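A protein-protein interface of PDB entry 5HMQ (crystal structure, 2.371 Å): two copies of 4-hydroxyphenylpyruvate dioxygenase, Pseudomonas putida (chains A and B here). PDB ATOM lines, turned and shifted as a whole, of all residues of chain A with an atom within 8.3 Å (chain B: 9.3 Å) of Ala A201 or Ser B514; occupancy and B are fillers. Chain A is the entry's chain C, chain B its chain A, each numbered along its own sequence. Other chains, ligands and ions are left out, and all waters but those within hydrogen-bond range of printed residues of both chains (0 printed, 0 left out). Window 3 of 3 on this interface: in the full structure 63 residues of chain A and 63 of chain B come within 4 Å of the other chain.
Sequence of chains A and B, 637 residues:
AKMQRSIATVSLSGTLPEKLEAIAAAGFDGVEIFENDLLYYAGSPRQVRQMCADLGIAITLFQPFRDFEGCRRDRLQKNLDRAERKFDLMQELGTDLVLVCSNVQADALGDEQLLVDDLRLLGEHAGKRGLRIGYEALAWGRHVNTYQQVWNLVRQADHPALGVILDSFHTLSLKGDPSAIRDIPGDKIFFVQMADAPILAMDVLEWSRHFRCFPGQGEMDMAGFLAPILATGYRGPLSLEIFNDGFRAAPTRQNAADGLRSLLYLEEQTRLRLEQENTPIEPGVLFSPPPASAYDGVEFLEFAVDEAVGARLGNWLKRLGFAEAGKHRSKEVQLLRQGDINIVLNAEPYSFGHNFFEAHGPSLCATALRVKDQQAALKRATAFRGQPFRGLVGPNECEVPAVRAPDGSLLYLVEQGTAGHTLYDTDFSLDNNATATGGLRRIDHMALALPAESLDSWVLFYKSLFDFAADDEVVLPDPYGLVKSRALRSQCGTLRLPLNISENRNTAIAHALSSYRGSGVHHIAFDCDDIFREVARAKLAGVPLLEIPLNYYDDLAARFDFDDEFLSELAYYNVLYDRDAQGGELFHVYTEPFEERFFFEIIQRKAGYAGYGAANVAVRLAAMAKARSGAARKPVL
Among the printed residues, pairs that only touch across the chains: Pro A198 with Ile B509 (3.9 Å), Ala A201 with Ser B514 (3.5 Å), Met A202 with Ser B514 (3.4 Å), Met A202 with Tyr B516 (3.6 Å), Met A202 with Arg B517 (3.2 Å), Phe A211 with Ile B509 (3.4 Å) and Phe A211 with Tyr B516 (3.8 Å).
The guanidinium group (NE) of Arg B517 lies within salt-bridge range of the side-chain carboxylate (OE1) of Glu A206 (3.7 Å).
NE1 of Trp A207 is in hydrogen-bond range of O of Pro A198. The backbone NH (N) of Glu A206 lies within hydrogen-bond range of the side-chain carboxylate (OD2) of Asp A203, 3.4 Å away.
No position is printed for both chains.
Printed residues of chain A that touch a printed residue of chain B: Pro A198, Ala A201, Met A202, Glu A206 and Phe A211. Hydrophobic or aromatic side chains of chain B that line the printed part of chain A: Ile B509 and Tyr B516. Among the printed residues, 8 pairs touch across the chains. Among the printed residues, Asp or Glu carboxylates within 4 Å of a Lys or Arg side-chain nitrogen of the other chain: Glu A206 with Arg B517 (3.7 Å).
Ala A201 touches one residue of chain B. Ser B514 touches two residues of chain A. Of chain B, only Ser B514 (3.4 Å), Tyr B516 (3.6 Å) and Arg B517 (3.2 Å) come within 4 Å of Met A202. Printed residues of chain B within 4 Å of Pro A198: Ile B509 (3.9 Å). Of the printed residues of chain B, Phe A211 touches Ile B509 (3.4 Å) and Tyr B516 (3.8 Å). The nearest residue of chain B that does not touch Ala A201 is Leu B513 (5.4 Å). The nearest printed residue of chain A that does not touch Tyr B516 is Glu A206 (4.5 Å).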
ATOM      1  N   SER A 173     -21.601 -33.262  -1.517  1.00  0.00           N
ATOM      2  CA  SER A 173     -21.388 -32.643  -0.211  1.00  0.00           C
ATOM      3  C   SER A 173     -20.471 -33.484   0.666  1.00  0.00           C
ATOM      4  O   SER A 173     -19.767 -32.942   1.525  1.00  0.00           O
ATOM      5  CB  SER A 173     -22.722 -32.416   0.500  1.00  0.00           C
ATOM      6  OG  SER A 173     -23.368 -33.647   0.779  1.00  0.00           O
ATOM      7  N   PRO A 198     -22.776 -23.790  -2.397  1.00  0.00           N
ATOM      8  CA  PRO A 198     -21.421 -23.384  -2.020  1.00  0.00           C
ATOM      9  C   PRO A 198     -20.766 -24.442  -1.147  1.00  0.00           C
ATOM     10  O   PRO A 198     -21.432 -25.157  -0.395  1.00  0.00           O
ATOM     11  CB  PRO A 198     -21.644 -22.081  -1.245  1.00  0.00           C
ATOM     12  CG  PRO A 198     -23.014 -22.233  -0.677  1.00  0.00           C
ATOM     13  CD  PRO A 198     -23.801 -22.969  -1.729  1.00  0.00           C
ATOM     14  N   ILE A 199     -19.445 -24.543  -1.260  1.00  0.00           N
ATOM     15  CA  ILE A 199     -18.689 -25.478  -0.434  1.00  0.00           C
ATOM     16  C   ILE A 199     -18.523 -24.862   0.949  1.00  0.00           C
ATOM     17  O   ILE A 199     -17.873 -23.822   1.106  1.00  0.00           O
ATOM     18  CB  ILE A 199     -17.329 -25.810  -1.060  1.00  0.00           C
ATOM     19  CG1 ILE A 199     -17.510 -26.368  -2.471  1.00  0.00           C
ATOM     20  CG2 ILE A 199     -16.600 -26.828  -0.202  1.00  0.00           C
ATOM     21  CD1 ILE A 199     -18.435 -27.566  -2.557  1.00  0.00           C
ATOM     22  N   LEU A 200     -19.120 -25.500   1.956  1.00  0.00           N
ATOM     23  CA  LEU A 200     -19.126 -24.989   3.316  1.00  0.00           C
ATOM     24  C   LEU A 200     -18.727 -26.084   4.292  1.00  0.00           C
ATOM     25  O   LEU A 200     -19.148 -27.236   4.148  1.00  0.00           O
ATOM     26  CB  LEU A 200     -20.518 -24.441   3.671  1.00  0.00           C
ATOM     27  CG  LEU A 200     -21.026 -23.307   2.785  1.00  0.00           C
ATOM     28  CD1 LEU A 200     -22.528 -23.120   2.971  1.00  0.00           C
ATOM     29  CD2 LEU A 200     -20.283 -22.013   3.134  1.00  0.00           C
ATOM     30  N   ALA A 201     -17.927 -25.716   5.295  1.00  0.00           N
ATOM     31  CA  ALA A 201     -17.550 -26.639   6.364  1.00  0.00           C
ATOM     32  C   ALA A 201     -18.675 -26.642   7.397  1.00  0.00           C
ATOM     33  O   ALA A 201     -18.581 -26.080   8.490  1.00  0.00           O
ATOM     34  CB  ALA A 201     -16.214 -26.248   6.976  1.00  0.00           C
ATOM     35  N   MET A 202     -19.767 -27.288   7.015  1.00  0.00           N
ATOM     36  CA  MET A 202     -21.023 -27.171   7.735  1.00  0.00           C
ATOM     37  C   MET A 202     -21.665 -28.535   7.922  1.00  0.00           C
ATOM     38  O   MET A 202     -21.418 -29.449   7.135  1.00  0.00           O
ATOM     39  CB  MET A 202     -21.960 -26.236   6.969  1.00  0.00           C
ATOM     40  CG  MET A 202     -23.242 -25.864   7.676  1.00  0.00           C
ATOM     41  SD  MET A 202     -24.269 -24.678   6.534  1.00  0.00           S
ATOM     42  CE  MET A 202     -25.726 -24.258   7.743  1.00  0.00           C
ATOM     43  N   ASP A 203     -22.470 -28.677   8.972  1.00  0.00           N
ATOM     44  CA  ASP A 203     -23.290 -29.869   9.125  1.00  0.00           C
ATOM     45  C   ASP A 203     -24.090 -30.091   7.851  1.00  0.00           C
ATOM     46  O   ASP A 203     -24.821 -29.201   7.405  1.00  0.00           O
ATOM     47  CB  ASP A 203     -24.219 -29.708  10.332  1.00  0.00           C
ATOM     48  CG  ASP A 203     -25.129 -30.902  10.535  1.00  0.00           C
ATOM     49  OD1 ASP A 203     -24.625 -31.973  10.935  1.00  0.00           O
ATOM     50  OD2 ASP A 203     -26.349 -30.767  10.296  1.00  0.00           O
ATOM     51  N   VAL A 204     -23.946 -31.283   7.265  1.00  0.00           N
ATOM     52  CA  VAL A 204     -24.468 -31.516   5.921  1.00  0.00           C
ATOM     53  C   VAL A 204     -25.986 -31.390   5.892  1.00  0.00           C
ATOM     54  O   VAL A 204     -26.563 -30.974   4.880  1.00  0.00           O
ATOM     55  CB  VAL A 204     -23.986 -32.882   5.394  1.00  0.00           C
ATOM     56  CG1 VAL A 204     -24.397 -33.065   3.951  1.00  0.00           C
ATOM     57  CG2 VAL A 204     -22.475 -32.979   5.516  1.00  0.00           C
ATOM     58  N   GLU A 206     -27.866 -29.238   7.713  1.00  0.00           N
ATOM     59  CA  GLU A 206     -28.160 -27.811   7.618  1.00  0.00           C
ATOM     60  C   GLU A 206     -27.638 -27.228   6.312  1.00  0.00           C
ATOM     61  O   GLU A 206     -28.257 -26.319   5.747  1.00  0.00           O
ATOM     62  CB  GLU A 206     -27.554 -27.075   8.814  1.00  0.00           C
ATOM     63  CG  GLU A 206     -27.886 -27.680  10.172  1.00  0.00           C
ATOM     64  CD  GLU A 206     -29.303 -27.381  10.626  1.00  0.00           C
ATOM     65  OE1 GLU A 206     -29.921 -26.437  10.087  1.00  0.00           O
ATOM     66  OE2 GLU A 206     -29.797 -28.092  11.527  1.00  0.00           O
ATOM     67  N   TRP A 207     -26.505 -27.740   5.826  1.00  0.00           N
ATOM     68  CA  TRP A 207     -25.984 -27.347   4.520  1.00  0.00           C
ATOM     69  C   TRP A 207     -26.998 -27.625   3.416  1.00  0.00           C
ATOM     70  O   TRP A 207     -27.215 -26.785   2.533  1.00  0.00           O
ATOM     71  CB  TRP A 207     -24.671 -28.093   4.269  1.00  0.00           C
ATOM     72  CG  TRP A 207     -23.902 -27.715   3.036  1.00  0.00           C
ATOM     73  CD1 TRP A 207     -24.173 -26.701   2.165  1.00  0.00           C
ATOM     74  CD2 TRP A 207     -22.713 -28.352   2.553  1.00  0.00           C
ATOM     75  NE1 TRP A 207     -23.232 -26.676   1.162  1.00  0.00           N
ATOM     76  CE2 TRP A 207     -22.325 -27.680   1.379  1.00  0.00           C
ATOM     77  CE3 TRP A 207     -21.942 -29.431   2.999  1.00  0.00           C
ATOM     78  CZ2 TRP A 207     -21.198 -28.049   0.646  1.00  0.00           C
ATOM     79  CZ3 TRP A 207     -20.826 -29.797   2.270  1.00  0.00           C
ATOM     80  CH2 TRP A 207     -20.465 -29.108   1.107  1.00  0.00           C
ATOM     81  N   PHE A 211     -28.792 -24.088   1.707  1.00  0.00           N
ATOM     82  CA  PHE A 211     -27.864 -23.551   0.714  1.00  0.00           C
ATOM     83  C   PHE A 211     -27.899 -24.234  -0.646  1.00  0.00           C
ATOM     84  O   PHE A 211     -27.028 -23.955  -1.479  1.00  0.00           O
ATOM     85  CB  PHE A 211     -26.441 -23.556   1.273  1.00  0.00           C
ATOM     86  CG  PHE A 211     -26.269 -22.651   2.451  1.00  0.00           C
ATOM     87  CD1 PHE A 211     -26.024 -21.303   2.263  1.00  0.00           C
ATOM     88  CD2 PHE A 211     -26.381 -23.134   3.741  1.00  0.00           C
ATOM     89  CE1 PHE A 211     -25.880 -20.453   3.340  1.00  0.00           C
ATOM     90  CE2 PHE A 211     -26.234 -22.287   4.822  1.00  0.00           C
ATOM     91  CZ  PHE A 211     -25.983 -20.943   4.620  1.00  0.00           C
ATOM     92  N   THR B 507     -25.158 -13.903   3.268  1.00  0.00           N
ATOM     93  CA  THR B 507     -24.192 -13.289   4.175  1.00  0.00           C
ATOM     94  C   THR B 507     -23.433 -14.340   4.978  1.00  0.00           C
ATOM     95  O   THR B 507     -22.234 -14.180   5.237  1.00  0.00           O
ATOM     96  CB  THR B 507     -24.897 -12.304   5.110  1.00  0.00           C
ATOM     97  OG1 THR B 507     -25.445 -11.225   4.340  1.00  0.00           O
ATOM     98  CG2 THR B 507     -23.924 -11.737   6.138  1.00  0.00           C
ATOM     99  N   ALA B 508     -24.108 -15.426   5.373  1.00  0.00           N
ATOM    100  CA  ALA B 508     -23.396 -16.552   5.968  1.00  0.00           C
ATOM    101  C   ALA B 508     -22.417 -17.141   4.970  1.00  0.00           C
ATOM    102  O   ALA B 508     -21.362 -17.660   5.358  1.00  0.00           O
ATOM    103  CB  ALA B 508     -24.381 -17.620   6.445  1.00  0.00           C
ATOM    104  N   ILE B 509     -22.750 -17.058   3.682  1.00  0.00           N
ATOM    105  CA  ILE B 509     -21.820 -17.484   2.648  1.00  0.00           C
ATOM    106  C   ILE B 509     -20.683 -16.474   2.546  1.00  0.00           C
ATOM    107  O   ILE B 509     -19.509 -16.851   2.615  1.00  0.00           O
ATOM    108  CB  ILE B 509     -22.562 -17.678   1.309  1.00  0.00           C
ATOM    109  CG1 ILE B 509     -23.724 -18.649   1.481  1.00  0.00           C
ATOM    110  CG2 ILE B 509     -21.679 -18.282   0.238  1.00  0.00           C
ATOM    111  CD1 ILE B 509     -24.598 -18.763   0.261  1.00  0.00           C
ATOM    112  N   HIS B 511     -19.274 -14.557   4.602  1.00  0.00           N
ATOM    113  CA  HIS B 511     -18.302 -14.769   5.663  1.00  0.00           C
ATOM    114  C   HIS B 511     -17.791 -16.199   5.570  1.00  0.00           C
ATOM    115  O   HIS B 511     -17.649 -16.747   4.469  1.00  0.00           O
ATOM    116  CB  HIS B 511     -18.927 -14.538   7.037  1.00  0.00           C
ATOM    117  CG  HIS B 511     -19.442 -13.132   7.260  1.00  0.00           C
ATOM    118  ND1 HIS B 511     -20.134 -12.418   6.279  1.00  0.00           N
ATOM    119  CD2 HIS B 511     -19.418 -12.342   8.367  1.00  0.00           C
ATOM    120  CE1 HIS B 511     -20.469 -11.236   6.757  1.00  0.00           C
ATOM    121  NE2 HIS B 511     -20.054 -11.170   8.018  1.00  0.00           N
ATOM    122  N   ALA B 512     -17.468 -16.795   6.711  1.00  0.00           N
ATOM    123  CA  ALA B 512     -17.073 -18.185   6.776  1.00  0.00           C
ATOM    124  C   ALA B 512     -17.930 -18.893   7.803  1.00  0.00           C
ATOM    125  O   ALA B 512     -17.458 -19.757   8.545  1.00  0.00           O
ATOM    126  CB  ALA B 512     -15.590 -18.321   7.110  1.00  0.00           C
ATOM    127  N   LEU B 513     -19.210 -18.550   7.858  1.00  0.00           N
ATOM    128  CA  LEU B 513     -20.034 -19.102   8.918  1.00  0.00           C
ATOM    129  C   LEU B 513     -20.296 -20.587   8.715  1.00  0.00           C
ATOM    130  O   LEU B 513     -20.371 -21.091   7.589  1.00  0.00           O
ATOM    131  CB  LEU B 513     -21.363 -18.346   9.012  1.00  0.00           C
ATOM    132  CG  LEU B 513     -21.266 -16.944   9.616  1.00  0.00           C
ATOM    133  CD1 LEU B 513     -22.622 -16.254   9.608  1.00  0.00           C
ATOM    134  CD2 LEU B 513     -20.688 -17.048  11.018  1.00  0.00           C
ATOM    135  N   SER B 514     -20.455 -21.276   9.838  1.00  0.00           N
ATOM    136  CA  SER B 514     -20.763 -22.694   9.875  1.00  0.00           C
ATOM    137  C   SER B 514     -22.070 -23.001  10.598  1.00  0.00           C
ATOM    138  O   SER B 514     -22.580 -24.121  10.472  1.00  0.00           O
ATOM    139  CB  SER B 514     -19.612 -23.459  10.549  1.00  0.00           C
ATOM    140  OG  SER B 514     -19.671 -23.235  11.949  1.00  0.00           O
ATOM    141  N   SER B 515     -22.597 -22.062  11.381  1.00  0.00           N
ATOM    142  CA  SER B 515     -23.907 -22.174  12.016  1.00  0.00           C
ATOM    143  C   SER B 515     -24.862 -21.088  11.527  1.00  0.00           C
ATOM    144  O   SER B 515     -25.025 -20.056  12.184  1.00  0.00           O
ATOM    145  CB  SER B 515     -23.719 -22.104  13.522  1.00  0.00           C
ATOM    146  OG  SER B 515     -23.263 -20.815  13.904  1.00  0.00           O
ATOM    147  N   TYR B 516     -25.558 -21.351  10.424  1.00  0.00           N
ATOM    148  CA  TYR B 516     -26.611 -20.466   9.935  1.00  0.00           C
ATOM    149  C   TYR B 516     -27.939 -21.185  10.114  1.00  0.00           C
ATOM    150  O   TYR B 516     -28.096 -22.322   9.660  1.00  0.00           O
ATOM    151  CB  TYR B 516     -26.415 -20.091   8.459  1.00  0.00           C
ATOM    152  CG  TYR B 516     -27.650 -19.459   7.821  1.00  0.00           C
ATOM    153  CD1 TYR B 516     -28.668 -20.251   7.287  1.00  0.00           C
ATOM    154  CD2 TYR B 516     -27.799 -18.079   7.747  1.00  0.00           C
ATOM    155  CE1 TYR B 516     -29.793 -19.691   6.717  1.00  0.00           C
ATOM    156  CE2 TYR B 516     -28.925 -17.509   7.169  1.00  0.00           C
ATOM    157  CZ  TYR B 516     -29.917 -18.322   6.655  1.00  0.00           C
ATOM    158  OH  TYR B 516     -31.038 -17.767   6.081  1.00  0.00           O
ATOM    159  N   ARG B 517     -28.895 -20.523  10.762  1.00  0.00           N
ATOM    160  CA  ARG B 517     -30.136 -21.181  11.142  1.00  0.00           C
ATOM    161  C   ARG B 517     -31.393 -20.479  10.645  1.00  0.00           C
ATOM    162  O   ARG B 517     -32.495 -20.989  10.878  1.00  0.00           O
ATOM    163  CB  ARG B 517     -30.184 -21.356  12.669  1.00  0.00           C
ATOM    164  CG  ARG B 517     -29.156 -22.362  13.176  1.00  0.00           C
ATOM    165  CD  ARG B 517     -29.203 -23.657  12.359  1.00  0.00           C
ATOM    166  NE  ARG B 517     -28.078 -24.552  12.635  1.00  0.00           N
ATOM    167  CZ  ARG B 517     -27.000 -24.664  11.864  1.00  0.00           C
ATOM    168  NH1 ARG B 517     -26.891 -23.941  10.760  1.00  0.00           N
ATOM    169  NH2 ARG B 517     -26.028 -25.505  12.192  1.00  0.00           N
ATOM    170  N   GLU B 596     -28.591 -22.983  19.023  1.00  0.00           N
ATOM    171  CA  GLU B 596     -28.315 -21.980  17.995  1.00  0.00           C
ATOM    172  C   GLU B 596     -29.577 -21.390  17.370  1.00  0.00           C
ATOM    173  O   GLU B 596     -29.524 -20.860  16.254  1.00  0.00           O
ATOM    174  CB  GLU B 596     -27.406 -22.541  16.891  1.00  0.00           C
ATOM    175  CG  GLU B 596     -25.978 -22.817  17.332  1.00  0.00           C
ATOM    176  CD  GLU B 596     -25.821 -24.166  18.004  1.00  0.00           C
ATOM    177  OE1 GLU B 596     -26.508 -25.124  17.588  1.00  0.00           O
ATOM    178  OE2 GLU B 596     -25.009 -24.269  18.947  1.00  0.00           O
